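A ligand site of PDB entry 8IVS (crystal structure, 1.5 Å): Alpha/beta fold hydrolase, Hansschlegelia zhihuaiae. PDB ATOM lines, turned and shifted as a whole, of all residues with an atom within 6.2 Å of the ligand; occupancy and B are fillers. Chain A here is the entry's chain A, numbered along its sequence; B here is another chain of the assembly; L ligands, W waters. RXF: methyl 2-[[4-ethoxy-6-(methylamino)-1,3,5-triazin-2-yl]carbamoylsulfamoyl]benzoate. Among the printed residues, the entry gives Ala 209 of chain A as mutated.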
ATOM      1  N   GLY A  77     -18.574  23.304 -13.723  1.00  0.00           N
ATOM      2  CA  GLY A  77     -19.851  23.413 -13.042  1.00  0.00           C
ATOM      3  C   GLY A  77     -19.822  24.379 -11.866  1.00  0.00           C
ATOM      4  O   GLY A  77     -18.894  25.173 -11.683  1.00  0.00           O
ATOM      5  N   GLY A  78     -20.873  24.297 -11.064  1.00  0.00           N
ATOM      6  CA  GLY A  78     -21.094  25.285 -10.032  1.00  0.00           C
ATOM      7  C   GLY A  78     -20.032  25.211  -8.943  1.00  0.00           C
ATOM      8  O   GLY A  78     -19.730  24.126  -8.430  1.00  0.00           O
ATOM      9  N   GLY A  79     -19.494  26.366  -8.578  1.00  0.00           N
ATOM     10  CA  GLY A  79     -18.499  26.421  -7.521  1.00  0.00           C
ATOM     11  C   GLY A  79     -17.157  25.849  -7.880  1.00  0.00           C
ATOM     12  O   GLY A  79     -16.353  25.579  -6.985  1.00  0.00           O
ATOM     13  N   LEU A  80     -16.866  25.695  -9.171  1.00  0.00           N
ATOM     14  CA  LEU A  80     -15.648  25.010  -9.620  1.00  0.00           C
ATOM     15  C   LEU A  80     -14.796  25.950 -10.464  1.00  0.00           C
ATOM     16  O   LEU A  80     -15.077  27.150 -10.586  1.00  0.00           O
ATOM     17  CB  LEU A  80     -16.016  23.731 -10.393  1.00  0.00           C
ATOM     18  CG  LEU A  80     -16.805  22.709  -9.563  1.00  0.00           C
ATOM     19  CD1 LEU A  80     -17.566  21.741 -10.461  1.00  0.00           C
ATOM     20  CD2 LEU A  80     -15.877  21.962  -8.613  1.00  0.00           C
ATOM     21  N   SER A 142     -21.658  25.445  -0.563  1.00  0.00           N
ATOM     22  CA  SER A 142     -21.908  24.062  -0.179  1.00  0.00           C
ATOM     23  C   SER A 142     -20.898  23.581   0.861  1.00  0.00           C
ATOM     24  O   SER A 142     -19.741  23.977   0.863  1.00  0.00           O
ATOM     25  CB  SER A 142     -21.849  23.123  -1.390  1.00  0.00           C
ATOM     26  OG  SER A 142     -22.264  21.813  -0.993  1.00  0.00           O
ATOM     27  N   ARG A 150     -24.791  15.752  -3.489  1.00  0.00           N
ATOM     28  CA  ARG A 150     -24.992  16.412  -4.777  1.00  0.00           C
ATOM     29  C   ARG A 150     -24.298  15.678  -5.908  1.00  0.00           C
ATOM     30  O   ARG A 150     -24.850  15.531  -6.995  1.00  0.00           O
ATOM     31  CB  ARG A 150     -24.502  17.850  -4.682  1.00  0.00           C
ATOM     32  CG  ARG A 150     -24.632  18.656  -5.979  1.00  0.00           C
ATOM     33  CD  ARG A 150     -23.768  19.893  -5.898  1.00  0.00           C
ATOM     34  NE  ARG A 150     -22.349  19.563  -6.000  1.00  0.00           N
ATOM     35  CZ  ARG A 150     -21.360  20.423  -5.744  1.00  0.00           C
ATOM     36  NH1 ARG A 150     -21.615  21.661  -5.340  1.00  0.00           N
ATOM     37  NH2 ARG A 150     -20.091  20.030  -5.891  1.00  0.00           N
ATOM     38  N   ASP A 151     -23.057  15.237  -5.683  1.00  0.00           N
ATOM     39  CA  ASP A 151     -22.260  14.635  -6.735  1.00  0.00           C
ATOM     40  C   ASP A 151     -22.423  13.129  -6.796  1.00  0.00           C
ATOM     41  O   ASP A 151     -21.798  12.464  -7.644  1.00  0.00           O
ATOM     42  CB  ASP A 151     -20.790  15.036  -6.545  1.00  0.00           C
ATOM     43  CG  ASP A 151     -20.581  16.564  -6.603  1.00  0.00           C
ATOM     44  OD1 ASP A 151     -21.477  17.271  -7.128  1.00  0.00           O
ATOM     45  OD2 ASP A 151     -19.532  17.054  -6.127  1.00  0.00           O
ATOM     46  N   HIS A 208     -21.018  21.379 -17.721  1.00  0.00           N
ATOM     47  CA  HIS A 208     -21.074  20.555 -16.523  1.00  0.00           C
ATOM     48  C   HIS A 208     -22.051  21.179 -15.534  1.00  0.00           C
ATOM     49  O   HIS A 208     -21.867  22.337 -15.158  1.00  0.00           O
ATOM     50  CB  HIS A 208     -19.693  20.454 -15.904  1.00  0.00           C
ATOM     51  CG  HIS A 208     -19.670  19.725 -14.594  1.00  0.00           C
ATOM     52  ND1 HIS A 208     -18.973  20.198 -13.505  1.00  0.00           N
ATOM     53  CD2 HIS A 208     -20.216  18.543 -14.222  1.00  0.00           C
ATOM     54  CE1 HIS A 208     -19.114  19.346 -12.506  1.00  0.00           C
ATOM     55  NE2 HIS A 208     -19.862  18.335 -12.907  1.00  0.00           N
ATOM     56  N   ALA A 209     -23.057  20.417 -15.098  1.00  0.00           N
ATOM     57  CA  ALA A 209     -23.930  20.827 -13.996  1.00  0.00           C
ATOM     58  C   ALA A 209     -24.435  22.260 -14.180  1.00  0.00           C
ATOM     59  O   ALA A 209     -25.183  22.521 -15.124  1.00  0.00           O
ATOM     60  CB  ALA A 209     -23.203  20.692 -12.672  1.00  0.00           C
ATOM     61  N   ALA A 210     -24.016  23.176 -13.309  1.00  0.00           N
ATOM     62  CA  ALA A 210     -24.500  24.556 -13.374  1.00  0.00           C
ATOM     63  C   ALA A 210     -24.258  25.220 -14.724  1.00  0.00           C
ATOM     64  O   ALA A 210     -25.023  26.116 -15.100  1.00  0.00           O
ATOM     65  CB  ALA A 210     -23.859  25.403 -12.280  1.00  0.00           C
ATOM     66  N   SER A 211     -23.193  24.848 -15.455  1.00  0.00           N
ATOM     67  CA  SER A 211     -22.972  25.555 -16.708  1.00  0.00           C
ATOM     68  C   SER A 211     -23.782  24.956 -17.845  1.00  0.00           C
ATOM     69  O   SER A 211     -23.737  25.483 -18.964  1.00  0.00           O
ATOM     70  CB  SER A 211     -21.478  25.572 -17.125  1.00  0.00           C
ATOM     71  OG  SER A 211     -20.934  24.275 -17.360  1.00  0.00           O
ATOM     72  N   GLU A 232     -24.240  16.061 -16.846  1.00  0.00           N
ATOM     73  CA  GLU A 232     -25.077  16.217 -15.656  1.00  0.00           C
ATOM     74  C   GLU A 232     -25.628  17.647 -15.495  1.00  0.00           C
ATOM     75  O   GLU A 232     -25.478  18.253 -14.451  1.00  0.00           O
ATOM     76  CB  GLU A 232     -24.316  15.798 -14.409  1.00  0.00           C
ATOM     77  CG  GLU A 232     -23.797  14.380 -14.447  1.00  0.00           C
ATOM     78  CD  GLU A 232     -24.615  13.431 -13.614  1.00  0.00           C
ATOM     79  OE1 GLU A 232     -25.498  13.895 -12.860  1.00  0.00           O
ATOM     80  OE2 GLU A 232     -24.390  12.215 -13.706  1.00  0.00           O
ATOM     81  N   ALA A 234     -27.706  20.893 -14.608  1.00  0.00           N
ATOM     82  CA  ALA A 234     -28.460  21.105 -13.378  1.00  0.00           C
ATOM     83  C   ALA A 234     -29.815  21.772 -13.591  1.00  0.00           C
ATOM     84  O   ALA A 234     -30.719  21.576 -12.776  1.00  0.00           O
ATOM     85  CB  ALA A 234     -27.640  21.928 -12.373  1.00  0.00           C
ATOM     86  N   THR A 235     -29.973  22.609 -14.622  1.00  0.00           N
ATOM     87  CA  THR A 235     -31.221  23.325 -14.870  1.00  0.00           C
ATOM     88  C   THR A 235     -31.697  23.020 -16.277  1.00  0.00           C
ATOM     89  O   THR A 235     -30.926  23.132 -17.237  1.00  0.00           O
ATOM     90  CB  THR A 235     -31.045  24.843 -14.697  1.00  0.00           C
ATOM     91  OG1 THR A 235     -30.632  25.132 -13.355  1.00  0.00           O
ATOM     92  CG2 THR A 235     -32.355  25.569 -14.983  1.00  0.00           C
ATOM     93  N   PHE A 257     -34.976  22.605  -9.856  1.00  0.00           N
ATOM     94  CA  PHE A 257     -34.726  24.013 -10.172  1.00  0.00           C
ATOM     95  C   PHE A 257     -35.747  24.494 -11.192  1.00  0.00           C
ATOM     96  O   PHE A 257     -35.985  23.802 -12.180  1.00  0.00           O
ATOM     97  CB  PHE A 257     -33.308  24.219 -10.722  1.00  0.00           C
ATOM     98  CG  PHE A 257     -32.214  24.034  -9.706  1.00  0.00           C
ATOM     99  CD1 PHE A 257     -32.481  23.802  -8.365  1.00  0.00           C
ATOM    100  CD2 PHE A 257     -30.878  24.089 -10.111  1.00  0.00           C
ATOM    101  CE1 PHE A 257     -31.459  23.648  -7.436  1.00  0.00           C
ATOM    102  CE2 PHE A 257     -29.851  23.930  -9.190  1.00  0.00           C
ATOM    103  CZ  PHE A 257     -30.138  23.708  -7.856  1.00  0.00           C
ATOM    104  N   PRO A 258     -36.367  25.651 -10.982  1.00  0.00           N
ATOM    105  CA  PRO A 258     -37.327  26.161 -11.975  1.00  0.00           C
ATOM    106  C   PRO A 258     -36.698  26.193 -13.353  1.00  0.00           C
ATOM    107  O   PRO A 258     -35.618  26.781 -13.542  1.00  0.00           O
ATOM    108  CB  PRO A 258     -37.641  27.570 -11.456  1.00  0.00           C
ATOM    109  CG  PRO A 258     -37.486  27.437  -9.960  1.00  0.00           C
ATOM    110  CD  PRO A 258     -36.332  26.476  -9.768  1.00  0.00           C
ATOM    111  N   PHE A 293     -31.034  14.469  -2.686  1.00  0.00           N
ATOM    112  CA  PHE A 293     -30.353  14.743  -3.940  1.00  0.00           C
ATOM    113  C   PHE A 293     -30.457  13.618  -4.961  1.00  0.00           C
ATOM    114  O   PHE A 293     -30.426  13.844  -6.111  1.00  0.00           O
ATOM    115  CB  PHE A 293     -28.896  15.229  -3.700  1.00  0.00           C
ATOM    116  CG  PHE A 293     -28.609  16.596  -4.255  1.00  0.00           C
ATOM    117  CD1 PHE A 293     -28.854  16.878  -5.577  1.00  0.00           C
ATOM    118  CD2 PHE A 293     -28.099  17.584  -3.460  1.00  0.00           C
ATOM    119  CE1 PHE A 293     -28.583  18.134  -6.089  1.00  0.00           C
ATOM    120  CE2 PHE A 293     -27.849  18.838  -3.958  1.00  0.00           C
ATOM    121  CZ  PHE A 293     -28.095  19.112  -5.276  1.00  0.00           C
ATOM    122  N   TRP A 296     -33.751  14.335  -6.359  1.00  0.00           N
ATOM    123  CA  TRP A 296     -33.629  15.538  -7.173  1.00  0.00           C
ATOM    124  C   TRP A 296     -33.049  15.214  -8.547  1.00  0.00           C
ATOM    125  O   TRP A 296     -33.536  15.709  -9.568  1.00  0.00           O
ATOM    126  CB  TRP A 296     -32.771  16.559  -6.431  1.00  0.00           C
ATOM    127  CG  TRP A 296     -32.637  17.914  -7.065  1.00  0.00           C
ATOM    128  CD1 TRP A 296     -33.318  19.046  -6.746  1.00  0.00           C
ATOM    129  CD2 TRP A 296     -31.699  18.289  -8.092  1.00  0.00           C
ATOM    130  NE1 TRP A 296     -32.895  20.100  -7.535  1.00  0.00           N
ATOM    131  CE2 TRP A 296     -31.901  19.663  -8.362  1.00  0.00           C
ATOM    132  CE3 TRP A 296     -30.722  17.587  -8.822  1.00  0.00           C
ATOM    133  CZ2 TRP A 296     -31.160  20.356  -9.330  1.00  0.00           C
ATOM    134  CZ3 TRP A 296     -29.987  18.284  -9.783  1.00  0.00           C
ATOM    135  CH2 TRP A 296     -30.208  19.645 -10.017  1.00  0.00           C
ATOM    136  N   TRP A 297     -32.014  14.370  -8.587  1.00  0.00           N
ATOM    137  CA  TRP A 297     -31.426  13.987  -9.877  1.00  0.00           C
ATOM    138  C   TRP A 297     -32.403  13.163 -10.705  1.00  0.00           C
ATOM    139  O   TRP A 297     -32.420  13.283 -11.936  1.00  0.00           O
ATOM    140  CB  TRP A 297     -30.116  13.225  -9.637  1.00  0.00           C
ATOM    141  CG  TRP A 297     -28.930  14.139  -9.448  1.00  0.00           C
ATOM    142  CD1 TRP A 297     -28.158  14.268  -8.325  1.00  0.00           C
ATOM    143  CD2 TRP A 297     -28.406  15.055 -10.411  1.00  0.00           C
ATOM    144  NE1 TRP A 297     -27.171  15.207  -8.538  1.00  0.00           N
ATOM    145  CE2 TRP A 297     -27.301  15.698  -9.807  1.00  0.00           C
ATOM    146  CE3 TRP A 297     -28.740  15.398 -11.725  1.00  0.00           C
ATOM    147  CZ2 TRP A 297     -26.542  16.664 -10.472  1.00  0.00           C
ATOM    148  CZ3 TRP A 297     -27.988  16.360 -12.378  1.00  0.00           C
ATOM    149  CH2 TRP A 297     -26.906  16.975 -11.746  1.00  0.00           C
ATOM    150  N   PHE A 334     -19.318  13.918 -11.766  1.00  0.00           N
ATOM    151  CA  PHE A 334     -18.110  14.432 -12.428  1.00  0.00           C
ATOM    152  C   PHE A 334     -17.468  13.282 -13.198  1.00  0.00           C
ATOM    153  O   PHE A 334     -16.348  12.859 -12.879  1.00  0.00           O
ATOM    154  CB  PHE A 334     -17.060  14.964 -11.446  1.00  0.00           C
ATOM    155  CG  PHE A 334     -17.417  16.220 -10.669  1.00  0.00           C
ATOM    156  CD1 PHE A 334     -18.662  16.439 -10.116  1.00  0.00           C
ATOM    157  CD2 PHE A 334     -16.413  17.151 -10.404  1.00  0.00           C
ATOM    158  CE1 PHE A 334     -18.917  17.575  -9.369  1.00  0.00           C
ATOM    159  CE2 PHE A 334     -16.665  18.293  -9.645  1.00  0.00           C
ATOM    160  CZ  PHE A 334     -17.916  18.500  -9.116  1.00  0.00           C
ATOM    161  N   ILE B  43     -30.395  22.217  -0.964  1.00  0.00           N
ATOM    162  CA  ILE B  43     -30.275  23.554  -1.528  1.00  0.00           C
ATOM    163  C   ILE B  43     -31.561  24.305  -1.185  1.00  0.00           C
ATOM    164  O   ILE B  43     -32.638  23.737  -1.299  1.00  0.00           O
ATOM    165  CB  ILE B  43     -30.055  23.503  -3.048  1.00  0.00           C
ATOM    166  CG1 ILE B  43     -28.605  23.019  -3.283  1.00  0.00           C
ATOM    167  CG2 ILE B  43     -30.279  24.867  -3.704  1.00  0.00           C
ATOM    168  CD1 ILE B  43     -28.201  22.836  -4.708  1.00  0.00           C
ATOM    169  N   PRO B  44     -31.486  25.555  -0.682  1.00  0.00           N
ATOM    170  CA  PRO B  44     -30.281  26.362  -0.412  1.00  0.00           C
ATOM    171  C   PRO B  44     -29.294  25.732   0.579  1.00  0.00           C
ATOM    172  O   PRO B  44     -29.705  25.058   1.529  1.00  0.00           O
ATOM    173  CB  PRO B  44     -30.854  27.658   0.179  1.00  0.00           C
ATOM    174  CG  PRO B  44     -32.261  27.710  -0.303  1.00  0.00           C
ATOM    175  CD  PRO B  44     -32.717  26.287  -0.383  1.00  0.00           C
ATOM    176  N   TYR B  45     -28.005  25.917   0.322  1.00  0.00           N
ATOM    177  CA  TYR B  45     -26.972  25.301   1.157  1.00  0.00           C
ATOM    178  C   TYR B  45     -27.045  25.832   2.585  1.00  0.00           C
ATOM    179  O   TYR B  45     -27.421  26.978   2.830  1.00  0.00           O
ATOM    180  CB  TYR B  45     -25.587  25.557   0.565  1.00  0.00           C
ATOM    181  CG  TYR B  45     -25.344  24.897  -0.767  1.00  0.00           C
ATOM    182  CD1 TYR B  45     -25.371  23.509  -0.897  1.00  0.00           C
ATOM    183  CD2 TYR B  45     -25.061  25.647  -1.903  1.00  0.00           C
ATOM    184  CE1 TYR B  45     -25.146  22.898  -2.119  1.00  0.00           C
ATOM    185  CE2 TYR B  45     -24.835  25.054  -3.135  1.00  0.00           C
ATOM    186  CZ  TYR B  45     -24.871  23.663  -3.229  1.00  0.00           C
ATOM    187  OH  TYR B  45     -24.654  23.039  -4.435  1.00  0.00           O
HETATM  188  C1  RXF L   1     -30.839  27.381  -8.203  1.00  0.00           C
HETATM  189  C10 RXF L   1     -26.641  20.226  -9.031  1.00  0.00           C
HETATM  190  C11 RXF L   1     -25.328  20.423  -9.388  1.00  0.00           C
HETATM  191  C12 RXF L   1     -24.687  21.599  -9.044  1.00  0.00           C
HETATM  192  C13 RXF L   1     -23.277  21.740  -9.461  1.00  0.00           C
HETATM  193  C14 RXF L   1     -20.984  20.919  -9.344  1.00  0.00           C
HETATM  194  C2  RXF L   1     -29.934  27.867  -6.101  1.00  0.00           C
HETATM  195  C3  RXF L   1     -28.987  28.454  -4.101  1.00  0.00           C
HETATM  196  C4  RXF L   1     -30.207  30.073  -2.841  1.00  0.00           C
HETATM  197  C5  RXF L   1     -27.871  27.033  -5.548  1.00  0.00           C
HETATM  198  C6  RXF L   1     -26.482  25.578  -6.868  1.00  0.00           C
HETATM  199  C7  RXF L   1     -25.370  22.664  -8.293  1.00  0.00           C
HETATM  200  C8  RXF L   1     -26.687  22.396  -7.964  1.00  0.00           C
HETATM  201  C9  RXF L   1     -27.303  21.217  -8.329  1.00  0.00           C
HETATM  202  O3  RXF L   1     -24.521  24.948  -8.946  1.00  0.00           O
HETATM  203  O2  RXF L   1     -23.383  23.772  -7.321  1.00  0.00           O
HETATM  204  N   RXF L   1     -29.977  28.537  -4.961  1.00  0.00           N
HETATM  205  C   RXF L   1     -32.179  27.567  -8.802  1.00  0.00           C
HETATM  206  O   RXF L   1     -30.961  27.974  -6.948  1.00  0.00           O
HETATM  207  N1  RXF L   1     -29.105  29.145  -2.961  1.00  0.00           N
HETATM  208  N2  RXF L   1     -27.917  27.705  -4.384  1.00  0.00           N
HETATM  209  N3  RXF L   1     -26.780  26.291  -5.792  1.00  0.00           N
HETATM  210  N4  RXF L   1     -25.454  24.759  -6.693  1.00  0.00           N
HETATM  211  N5  RXF L   1     -28.883  27.117  -6.412  1.00  0.00           N
HETATM  212  O1  RXF L   1     -27.066  25.638  -7.914  1.00  0.00           O
HETATM  213  O4  RXF L   1     -22.934  22.591 -10.225  1.00  0.00           O
HETATM  214  O5  RXF L   1     -22.340  20.806  -8.946  1.00  0.00           O
HETATM  215  S   RXF L   1     -24.659  24.051  -7.861  1.00  0.00           S
HETATM  216  O   HOH W   1     -27.309  28.320  -1.147  1.00  0.00           O
HETATM  217  O   HOH W   2     -25.356  29.049  -2.838  1.00  0.00           O
HETATM  218  O   HOH W   3     -33.875  27.805 -11.779  1.00  0.00           O
HETATM  219  O   HOH W   4     -26.856  25.174 -10.788  1.00  0.00           O
HETATM  220  O   HOH W   5     -27.755  28.137  -9.221  1.00  0.00           O
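The guanidinium group of Arg 150 lies within hydrogen-bond range of an oxygen (O5) of the ligand (3.2 Å).
N of Gly 78 sits at hydrogen-bond distance from O4 of the ligand, 2.8 Å away.
OH of Tyr 45 of chain B sits at hydrogen-bond distance from N4 of the ligand, 2.9 Å away.
O4 of the ligand lies within hydrogen-bond range of N of Ala 210.
The backbone carbonyl oxygen of Arg 150 lies within hydrogen-bond range of the indole nitrogen of Trp 297, 2.8 Å away.
N of His 208 lies within hydrogen-bond range of OG of Ser 211 (2.9 Å).
The guanidinium group (NH1) of Arg 150 is in hydrogen-bond range of the side-chain hydroxyl (OH) of Tyr 45 of chain B, 3.5 Å away.
O of Ala 209 sits at hydrogen-bond distance from N of Ala 234.
The backbone carbonyl oxygen (O) of Glu 232 lies close to the backbone NH (N) of Ala 209, at 3.3 Å.
NE of Arg 150 is in salt-bridge range of OD1 of Asp 151, 2.7 Å away.
A ring nitrogen (ND1) of His 208 is in hydrogen-bond range of the backbone NH (N) of Gly 77, at 3.1 Å.
Residues that only touch the ligand: Gly 77, Leu 80, His 208, Ala 209, Ala 234, Phe 257, Phe 293, Trp 296, Trp 297, Phe 334, Ile 43 of chain B and Pro 44 of chain B.
Hydrophobic or aromatic side chains within 4 Å of the ligand: Leu 80, His 208, Ala 209, Ala 210, Ala 234, Phe 257, Phe 293, Trp 296, Trp 297, Phe 334, Ile 43 of chain B, Pro 44 of chain B and Tyr 45 of chain B.
The nearest printed residue that does not touch the ligand is Asp 151 (4.1 Å).
Water W1 lies within hydrogen-bond range of N1 of the ligand (2.7 Å) and N of Tyr 45 of chain B (2.9 Å).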
